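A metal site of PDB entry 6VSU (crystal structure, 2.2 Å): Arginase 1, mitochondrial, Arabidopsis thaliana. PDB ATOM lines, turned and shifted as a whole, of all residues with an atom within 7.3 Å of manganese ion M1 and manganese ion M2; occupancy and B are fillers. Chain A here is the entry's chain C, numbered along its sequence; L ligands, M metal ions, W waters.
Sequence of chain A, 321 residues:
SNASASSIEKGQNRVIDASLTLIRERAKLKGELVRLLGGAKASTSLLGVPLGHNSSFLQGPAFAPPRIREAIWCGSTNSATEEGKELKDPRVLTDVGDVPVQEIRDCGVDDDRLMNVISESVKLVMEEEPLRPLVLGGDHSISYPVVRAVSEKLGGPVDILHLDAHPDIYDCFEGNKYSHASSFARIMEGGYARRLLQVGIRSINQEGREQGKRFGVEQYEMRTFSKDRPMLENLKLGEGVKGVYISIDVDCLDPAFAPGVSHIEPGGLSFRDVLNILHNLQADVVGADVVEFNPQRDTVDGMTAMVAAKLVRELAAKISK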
ATOM      1  N   ASP A 139     -31.267  -9.705  28.032  1.00  0.00           N
ATOM      2  CA  ASP A 139     -30.160 -10.664  27.766  1.00  0.00           C
ATOM      3  C   ASP A 139     -29.934 -10.615  26.256  1.00  0.00           C
ATOM      4  O   ASP A 139     -30.761  -9.978  25.582  1.00  0.00           O
ATOM      5  CB  ASP A 139     -30.483 -12.020  28.388  1.00  0.00           C
ATOM      6  CG  ASP A 139     -31.476 -12.852  27.575  1.00  0.00           C
ATOM      7  OD1 ASP A 139     -31.506 -12.651  26.311  1.00  0.00           O
ATOM      8  OD2 ASP A 139     -32.114 -13.758  28.192  1.00  0.00           O
ATOM      9  N   HIS A 140     -28.791 -11.143  25.833  1.00  0.00           N
ATOM     10  CA  HIS A 140     -28.254 -11.079  24.445  1.00  0.00           C
ATOM     11  C   HIS A 140     -29.263 -11.597  23.412  1.00  0.00           C
ATOM     12  O   HIS A 140     -29.313 -11.038  22.338  1.00  0.00           O
ATOM     13  CB  HIS A 140     -26.853 -11.676  24.399  1.00  0.00           C
ATOM     14  CG  HIS A 140     -25.958 -10.697  23.739  1.00  0.00           C
ATOM     15  ND1 HIS A 140     -24.670 -10.457  24.064  1.00  0.00           N
ATOM     16  CD2 HIS A 140     -26.238  -9.811  22.786  1.00  0.00           C
ATOM     17  CE1 HIS A 140     -24.218  -9.511  23.299  1.00  0.00           C
ATOM     18  NE2 HIS A 140     -25.148  -9.100  22.533  1.00  0.00           N
ATOM     19  N   SER A 141     -30.042 -12.604  23.798  1.00  0.00           N
ATOM     20  CA  SER A 141     -31.127 -13.213  22.977  1.00  0.00           C
ATOM     21  C   SER A 141     -31.895 -12.155  22.172  1.00  0.00           C
ATOM     22  O   SER A 141     -32.238 -12.505  21.045  1.00  0.00           O
ATOM     23  CB  SER A 141     -32.084 -14.105  23.774  1.00  0.00           C
ATOM     24  OG  SER A 141     -33.168 -13.417  24.393  1.00  0.00           O
ATOM     25  N   SER A 143     -31.003  -9.400  20.574  1.00  0.00           N
ATOM     26  CA  SER A 143     -30.305  -8.812  19.408  1.00  0.00           C
ATOM     27  C   SER A 143     -30.842  -9.422  18.099  1.00  0.00           C
ATOM     28  O   SER A 143     -30.995  -8.665  17.078  1.00  0.00           O
ATOM     29  CB  SER A 143     -28.850  -9.004  19.575  1.00  0.00           C
ATOM     30  OG  SER A 143     -28.486  -8.664  20.907  1.00  0.00           O
ATOM     31  N   HIS A 162     -20.097  -5.660  17.466  1.00  0.00           N
ATOM     32  CA  HIS A 162     -20.533  -6.514  18.583  1.00  0.00           C
ATOM     33  C   HIS A 162     -19.401  -6.514  19.612  1.00  0.00           C
ATOM     34  O   HIS A 162     -18.357  -7.155  19.347  1.00  0.00           O
ATOM     35  CB  HIS A 162     -20.873  -7.888  18.042  1.00  0.00           C
ATOM     36  CG  HIS A 162     -21.231  -8.864  19.097  1.00  0.00           C
ATOM     37  ND1 HIS A 162     -20.996 -10.233  18.928  1.00  0.00           N
ATOM     38  CD2 HIS A 162     -21.777  -8.695  20.327  1.00  0.00           C
ATOM     39  CE1 HIS A 162     -21.419 -10.852  20.006  1.00  0.00           C
ATOM     40  NE2 HIS A 162     -21.884  -9.919  20.899  1.00  0.00           N
ATOM     41  N   LEU A 163     -19.565  -5.713  20.663  1.00  0.00           N
ATOM     42  CA  LEU A 163     -18.609  -5.543  21.781  1.00  0.00           C
ATOM     43  C   LEU A 163     -19.029  -6.509  22.889  1.00  0.00           C
ATOM     44  O   LEU A 163     -20.069  -6.262  23.470  1.00  0.00           O
ATOM     45  CB  LEU A 163     -18.703  -4.101  22.252  1.00  0.00           C
ATOM     46  CG  LEU A 163     -18.028  -3.089  21.351  1.00  0.00           C
ATOM     47  CD1 LEU A 163     -18.470  -1.691  21.670  1.00  0.00           C
ATOM     48  CD2 LEU A 163     -16.530  -3.214  21.470  1.00  0.00           C
ATOM     49  N   ASP A 164     -18.257  -7.588  23.111  1.00  0.00           N
ATOM     50  CA  ASP A 164     -18.638  -8.628  24.101  1.00  0.00           C
ATOM     51  C   ASP A 164     -17.447  -9.552  24.406  1.00  0.00           C
ATOM     52  O   ASP A 164     -16.579  -9.695  23.553  1.00  0.00           O
ATOM     53  CB  ASP A 164     -19.805  -9.447  23.552  1.00  0.00           C
ATOM     54  CG  ASP A 164     -20.424 -10.486  24.470  1.00  0.00           C
ATOM     55  OD1 ASP A 164     -19.746 -11.005  25.344  1.00  0.00           O
ATOM     56  OD2 ASP A 164     -21.502 -10.912  24.154  1.00  0.00           O
ATOM     57  N   ALA A 165     -17.390 -10.075  25.634  1.00  0.00           N
ATOM     58  CA  ALA A 165     -16.369 -11.056  26.071  1.00  0.00           C
ATOM     59  C   ALA A 165     -16.533 -12.375  25.313  1.00  0.00           C
ATOM     60  O   ALA A 165     -15.539 -13.070  25.094  1.00  0.00           O
ATOM     61  CB  ALA A 165     -16.447 -11.268  27.559  1.00  0.00           C
ATOM     62  N   HIS A 166     -17.793 -12.764  25.066  1.00  0.00           N
ATOM     63  CA  HIS A 166     -18.150 -14.020  24.361  1.00  0.00           C
ATOM     64  C   HIS A 166     -18.612 -13.658  22.945  1.00  0.00           C
ATOM     65  O   HIS A 166     -18.823 -12.509  22.663  1.00  0.00           O
ATOM     66  CB  HIS A 166     -19.280 -14.724  25.126  1.00  0.00           C
ATOM     67  CG  HIS A 166     -19.115 -14.629  26.606  1.00  0.00           C
ATOM     68  ND1 HIS A 166     -19.394 -13.469  27.298  1.00  0.00           N
ATOM     69  CD2 HIS A 166     -18.702 -15.529  27.510  1.00  0.00           C
ATOM     70  CE1 HIS A 166     -19.148 -13.670  28.573  1.00  0.00           C
ATOM     71  NE2 HIS A 166     -18.737 -14.931  28.729  1.00  0.00           N
ATOM     72  N   PRO A 167     -18.668 -14.630  22.004  1.00  0.00           N
ATOM     73  CA  PRO A 167     -19.101 -14.403  20.624  1.00  0.00           C
ATOM     74  C   PRO A 167     -20.550 -14.776  20.249  1.00  0.00           C
ATOM     75  O   PRO A 167     -21.038 -14.316  19.271  1.00  0.00           O
ATOM     76  CB  PRO A 167     -18.255 -15.398  19.820  1.00  0.00           C
ATOM     77  CG  PRO A 167     -17.749 -16.420  20.808  1.00  0.00           C
ATOM     78  CD  PRO A 167     -18.213 -15.985  22.186  1.00  0.00           C
ATOM     79  N   ASP A 168     -21.175 -15.609  21.066  1.00  0.00           N
ATOM     80  CA  ASP A 168     -22.616 -15.942  21.054  1.00  0.00           C
ATOM     81  C   ASP A 168     -23.117 -16.455  19.712  1.00  0.00           C
ATOM     82  O   ASP A 168     -24.217 -16.046  19.331  1.00  0.00           O
ATOM     83  CB  ASP A 168     -23.447 -14.724  21.438  1.00  0.00           C
ATOM     84  CG  ASP A 168     -23.098 -14.239  22.809  1.00  0.00           C
ATOM     85  OD1 ASP A 168     -22.635 -15.060  23.661  1.00  0.00           O
ATOM     86  OD2 ASP A 168     -23.289 -13.053  23.008  1.00  0.00           O
ATOM     87  N   HIS A 180     -29.049 -16.920  24.725  1.00  0.00           N
ATOM     88  CA  HIS A 180     -28.279 -15.642  24.586  1.00  0.00           C
ATOM     89  C   HIS A 180     -26.906 -15.912  23.950  1.00  0.00           C
ATOM     90  O   HIS A 180     -26.372 -14.964  23.344  1.00  0.00           O
ATOM     91  CB  HIS A 180     -28.214 -14.846  25.874  1.00  0.00           C
ATOM     92  CG  HIS A 180     -27.431 -15.458  26.980  1.00  0.00           C
ATOM     93  ND1 HIS A 180     -26.927 -14.681  28.024  1.00  0.00           N
ATOM     94  CD2 HIS A 180     -27.138 -16.747  27.278  1.00  0.00           C
ATOM     95  CE1 HIS A 180     -26.329 -15.456  28.880  1.00  0.00           C
ATOM     96  NE2 HIS A 180     -26.442 -16.739  28.457  1.00  0.00           N
ATOM     97  N   ALA A 181     -26.475 -17.185  23.980  1.00  0.00           N
ATOM     98  CA  ALA A 181     -25.191 -17.763  23.502  1.00  0.00           C
ATOM     99  C   ALA A 181     -25.265 -18.239  22.053  1.00  0.00           C
ATOM    100  O   ALA A 181     -24.240 -18.752  21.552  1.00  0.00           O
ATOM    101  CB  ALA A 181     -24.802 -18.922  24.399  1.00  0.00           C
ATOM    102  N   SER A 183     -27.316 -16.256  19.652  1.00  0.00           N
ATOM    103  CA  SER A 183     -28.032 -15.096  19.062  1.00  0.00           C
ATOM    104  C   SER A 183     -27.426 -14.701  17.721  1.00  0.00           C
ATOM    105  O   SER A 183     -28.195 -14.436  16.820  1.00  0.00           O
ATOM    106  CB  SER A 183     -28.017 -13.922  20.018  1.00  0.00           C
ATOM    107  OG  SER A 183     -28.279 -12.720  19.290  1.00  0.00           O
ATOM    108  N   PHE A 184     -26.095 -14.670  17.586  1.00  0.00           N
ATOM    109  CA  PHE A 184     -25.378 -14.203  16.362  1.00  0.00           C
ATOM    110  C   PHE A 184     -25.330 -15.317  15.334  1.00  0.00           C
ATOM    111  O   PHE A 184     -25.223 -14.984  14.180  1.00  0.00           O
ATOM    112  CB  PHE A 184     -24.028 -13.571  16.721  1.00  0.00           C
ATOM    113  CG  PHE A 184     -24.203 -12.189  17.297  1.00  0.00           C
ATOM    114  CD1 PHE A 184     -24.530 -12.021  18.632  1.00  0.00           C
ATOM    115  CD2 PHE A 184     -24.115 -11.059  16.494  1.00  0.00           C
ATOM    116  CE1 PHE A 184     -24.743 -10.748  19.161  1.00  0.00           C
ATOM    117  CE2 PHE A 184     -24.311  -9.801  17.033  1.00  0.00           C
ATOM    118  CZ  PHE A 184     -24.644  -9.636  18.352  1.00  0.00           C
ATOM    119  N   SER A 203     -13.597 -15.154  25.816  1.00  0.00           N
ATOM    120  CA  SER A 203     -14.322 -16.386  26.232  1.00  0.00           C
ATOM    121  C   SER A 203     -14.883 -16.959  24.948  1.00  0.00           C
ATOM    122  O   SER A 203     -15.922 -16.459  24.481  1.00  0.00           O
ATOM    123  CB  SER A 203     -15.389 -16.119  27.291  1.00  0.00           C
ATOM    124  OG  SER A 203     -15.771 -17.336  27.957  1.00  0.00           O
ATOM    125  N   SER A 247     -24.030  -3.794  18.903  1.00  0.00           N
ATOM    126  CA  SER A 247     -24.556  -4.600  20.005  1.00  0.00           C
ATOM    127  C   SER A 247     -23.545  -4.591  21.155  1.00  0.00           C
ATOM    128  O   SER A 247     -22.525  -5.261  21.021  1.00  0.00           O
ATOM    129  CB  SER A 247     -24.919  -5.978  19.589  1.00  0.00           C
ATOM    130  OG  SER A 247     -25.446  -6.706  20.665  1.00  0.00           O
ATOM    131  N   ILE A 248     -23.812  -3.811  22.201  1.00  0.00           N
ATOM    132  CA  ILE A 248     -22.842  -3.737  23.325  1.00  0.00           C
ATOM    133  C   ILE A 248     -23.287  -4.593  24.498  1.00  0.00           C
ATOM    134  O   ILE A 248     -24.209  -4.216  25.178  1.00  0.00           O
ATOM    135  CB  ILE A 248     -22.628  -2.289  23.788  1.00  0.00           C
ATOM    136  CG1 ILE A 248     -22.470  -1.342  22.610  1.00  0.00           C
ATOM    137  CG2 ILE A 248     -21.469  -2.200  24.739  1.00  0.00           C
ATOM    138  CD1 ILE A 248     -21.813  -0.063  22.968  1.00  0.00           C
ATOM    139  N   ASP A 249     -22.651  -5.754  24.641  1.00  0.00           N
ATOM    140  CA  ASP A 249     -22.846  -6.559  25.862  1.00  0.00           C
ATOM    141  C   ASP A 249     -21.979  -5.828  26.877  1.00  0.00           C
ATOM    142  O   ASP A 249     -20.810  -5.549  26.556  1.00  0.00           O
ATOM    143  CB  ASP A 249     -22.374  -7.988  25.698  1.00  0.00           C
ATOM    144  CG  ASP A 249     -22.539  -8.799  26.960  1.00  0.00           C
ATOM    145  OD1 ASP A 249     -22.671  -8.179  28.032  1.00  0.00           O
ATOM    146  OD2 ASP A 249     -22.474 -10.035  26.888  1.00  0.00           O
ATOM    147  N   VAL A 250     -22.507  -5.595  28.077  1.00  0.00           N
ATOM    148  CA  VAL A 250     -21.845  -4.806  29.158  1.00  0.00           C
ATOM    149  C   VAL A 250     -20.548  -5.476  29.636  1.00  0.00           C
ATOM    150  O   VAL A 250     -19.629  -4.751  29.906  1.00  0.00           O
ATOM    151  CB  VAL A 250     -22.840  -4.483  30.276  1.00  0.00           C
ATOM    152  CG1 VAL A 250     -22.147  -4.269  31.613  1.00  0.00           C
ATOM    153  CG2 VAL A 250     -23.660  -3.277  29.906  1.00  0.00           C
ATOM    154  N   ASP A 251     -20.437  -6.808  29.533  1.00  0.00           N
ATOM    155  CA  ASP A 251     -19.234  -7.587  29.911  1.00  0.00           C
ATOM    156  C   ASP A 251     -18.059  -7.429  28.917  1.00  0.00           C
ATOM    157  O   ASP A 251     -17.052  -8.102  29.141  1.00  0.00           O
ATOM    158  CB  ASP A 251     -19.591  -9.042  30.220  1.00  0.00           C
ATOM    159  CG  ASP A 251     -19.944  -9.839  28.994  1.00  0.00           C
ATOM    160  OD1 ASP A 251     -19.539  -9.421  27.905  1.00  0.00           O
ATOM    161  OD2 ASP A 251     -20.603 -10.869  29.134  1.00  0.00           O
ATOM    162  N   CYS A 252     -18.203  -6.681  27.819  1.00  0.00           N
ATOM    163  CA  CYS A 252     -17.041  -6.355  26.966  1.00  0.00           C
ATOM    164  C   CYS A 252     -16.032  -5.660  27.884  1.00  0.00           C
ATOM    165  O   CYS A 252     -14.853  -5.924  27.731  1.00  0.00           O
ATOM    166  CB  CYS A 252     -17.450  -5.518  25.758  1.00  0.00           C
ATOM    167  SG  CYS A 252     -17.871  -3.797  26.101  1.00  0.00           S
ATOM    168  N   HIS A 263     -21.899 -12.888  33.573  1.00  0.00           N
ATOM    169  CA  HIS A 263     -20.639 -13.603  33.280  1.00  0.00           C
ATOM    170  C   HIS A 263     -19.433 -12.707  33.559  1.00  0.00           C
ATOM    171  O   HIS A 263     -19.136 -11.853  32.726  1.00  0.00           O
ATOM    172  CB  HIS A 263     -20.672 -14.160  31.842  1.00  0.00           C
ATOM    173  CG  HIS A 263     -21.914 -14.940  31.554  1.00  0.00           C
ATOM    174  ND1 HIS A 263     -21.987 -16.276  31.798  1.00  0.00           N
ATOM    175  CD2 HIS A 263     -23.110 -14.570  31.068  1.00  0.00           C
ATOM    176  CE1 HIS A 263     -23.177 -16.698  31.462  1.00  0.00           C
ATOM    177  NE2 HIS A 263     -23.870 -15.685  31.022  1.00  0.00           N
ATOM    178  N   GLU A 265     -15.846 -12.087  33.394  1.00  0.00           N
ATOM    179  CA  GLU A 265     -14.726 -12.571  32.523  1.00  0.00           C
ATOM    180  C   GLU A 265     -13.566 -11.551  32.597  1.00  0.00           C
ATOM    181  O   GLU A 265     -13.508 -10.533  31.892  1.00  0.00           O
ATOM    182  CB  GLU A 265     -15.254 -12.879  31.126  1.00  0.00           C
ATOM    183  CG  GLU A 265     -14.258 -13.678  30.321  1.00  0.00           C
ATOM    184  CD  GLU A 265     -14.005 -15.115  30.743  1.00  0.00           C
ATOM    185  OE1 GLU A 265     -14.999 -15.800  31.188  1.00  0.00           O
ATOM    186  OE2 GLU A 265     -12.797 -15.554  30.617  1.00  0.00           O
ATOM    187  N   VAL A 291     -26.927  -4.486  26.372  1.00  0.00           N
ATOM    188  CA  VAL A 291     -27.530  -5.692  26.970  1.00  0.00           C
ATOM    189  C   VAL A 291     -26.651  -6.287  28.065  1.00  0.00           C
ATOM    190  O   VAL A 291     -25.557  -5.843  28.255  1.00  0.00           O
ATOM    191  CB  VAL A 291     -27.770  -6.752  25.862  1.00  0.00           C
ATOM    192  CG1 VAL A 291     -28.578  -6.203  24.706  1.00  0.00           C
ATOM    193  CG2 VAL A 291     -26.477  -7.351  25.336  1.00  0.00           C
ATOM    194  N   GLU A 292     -27.213  -7.261  28.765  1.00  0.00           N
ATOM    195  CA  GLU A 292     -26.516  -8.139  29.737  1.00  0.00           C
ATOM    196  C   GLU A 292     -26.179  -7.409  31.043  1.00  0.00           C
ATOM    197  O   GLU A 292     -25.585  -8.051  31.912  1.00  0.00           O
ATOM    198  CB  GLU A 292     -25.423  -8.945  29.036  1.00  0.00           C
ATOM    199  CG  GLU A 292     -26.000 -10.007  28.125  1.00  0.00           C
ATOM    200  CD  GLU A 292     -26.614 -11.207  28.814  1.00  0.00           C
ATOM    201  OE1 GLU A 292     -26.464 -11.333  30.032  1.00  0.00           O
ATOM    202  OE2 GLU A 292     -27.228 -12.045  28.129  1.00  0.00           O
HETATM  203  N1  LIG L   1     -21.017 -20.355  29.313  1.00  0.00           N
HETATM  204  C1  LIG L   1     -21.271 -19.600  28.058  1.00  0.00           C
HETATM  205  C2  LIG L   1     -21.437 -18.109  28.359  1.00  0.00           C
HETATM  206  C3  LIG L   1     -22.130 -17.307  27.278  1.00  0.00           C
HETATM  207  C4  LIG L   1     -22.547 -15.927  27.751  1.00  0.00           C
HETATM  208  N2  LIG L   1     -23.233 -15.085  26.759  1.00  0.00           N
HETATM  209  C5  LIG L   1     -20.134 -19.875  27.069  1.00  0.00           C
HETATM  210  O1  LIG L   1     -19.420 -20.865  27.291  1.00  0.00           O
HETATM  211  O2  LIG L   1     -20.017 -19.105  26.099  1.00  0.00           O
HETATM  212 MN    MN M   1     -23.398 -11.691  24.480  1.00  0.00          MN
HETATM  213 MN    MN M   2     -20.868 -11.722  26.944  1.00  0.00          MN
HETATM  214  O   HOH W   1     -24.869 -13.059  25.753  1.00  0.00           O
HETATM  215  O   HOH W   2     -22.422 -12.483  26.003  1.00  0.00           O
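OD1 of Asp 168 lies within salt-bridge range of N2 of the ligand, 3.2 Å away.
N of His 140 sits at hydrogen-bond distance from OE2 of Glu 292, at 2.9 Å.
A ring nitrogen (NE2) of His 140 sits at hydrogen-bond distance from the side-chain hydroxyl of Ser 247 (3.1 Å).
The backbone carbonyl oxygen (O) of His 140 lies within hydrogen-bond range of the side-chain hydroxyl (OG) of Ser 143, at 2.9 Å.
The backbone carbonyl oxygen (O) of Asp 168 is in hydrogen-bond range of the backbone NH (N) of Phe 184, at 2.9 Å.
The backbone carbonyl oxygen (O) of Asp 168 lies within hydrogen-bond range of the backbone NH (N) of Ser 183.
OD2 of Asp 164 sits close to NE2 of His 162, 3.4 Å away.
SG of Cys 252 sits at hydrogen-bond distance from O of Asp 249.
The side-chain carboxylate (OD1) of Asp 251 is in hydrogen-bond range of the backbone NH (N) of Ala 165 (3.2 Å).
Within 4 Å of manganese ion M1: His 140, Asp 164, Asp 168 and Asp 249.
The nearest printed residue that does not touch manganese ion M1 is His 162 (4.3 Å).
Of the 26 residues printed, 4 come within 4 Å of manganese ion M2.
Manganese ion M1 is bound by ND1 of His 140 (1.8 Å), water W2 (2.0 Å), OD2 of Asp 168 (2.0 Å), OD2 of Asp 164 (2.1 Å) and water W1 (2.4 Å).
Water W2 binds manganese ion M2 (2.0 Å).
Manganese ion M2 is bound by OD1 of Asp 164, at 2.1 Å.
Manganese ion M2 is bound by ND1 of His 166 (2.3 Å).
OD2 of Asp 249 is bound to manganese ion M2 (2.3 Å).
OD2 of Asp 251 is bound to manganese ion M2 (2.4 Å).
Slightly farther from manganese ion M2 lies the side-chain carboxylate (OD1) of Asp 251 (2.8 Å).
Water W1 lies within hydrogen-bond range of N2 of the ligand, O of His 180 and OE2 of Glu 292.
Water W2 bridges a nitrogen (N2) of the ligand and the side-chain carboxylate (OD1) of Asp 168.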
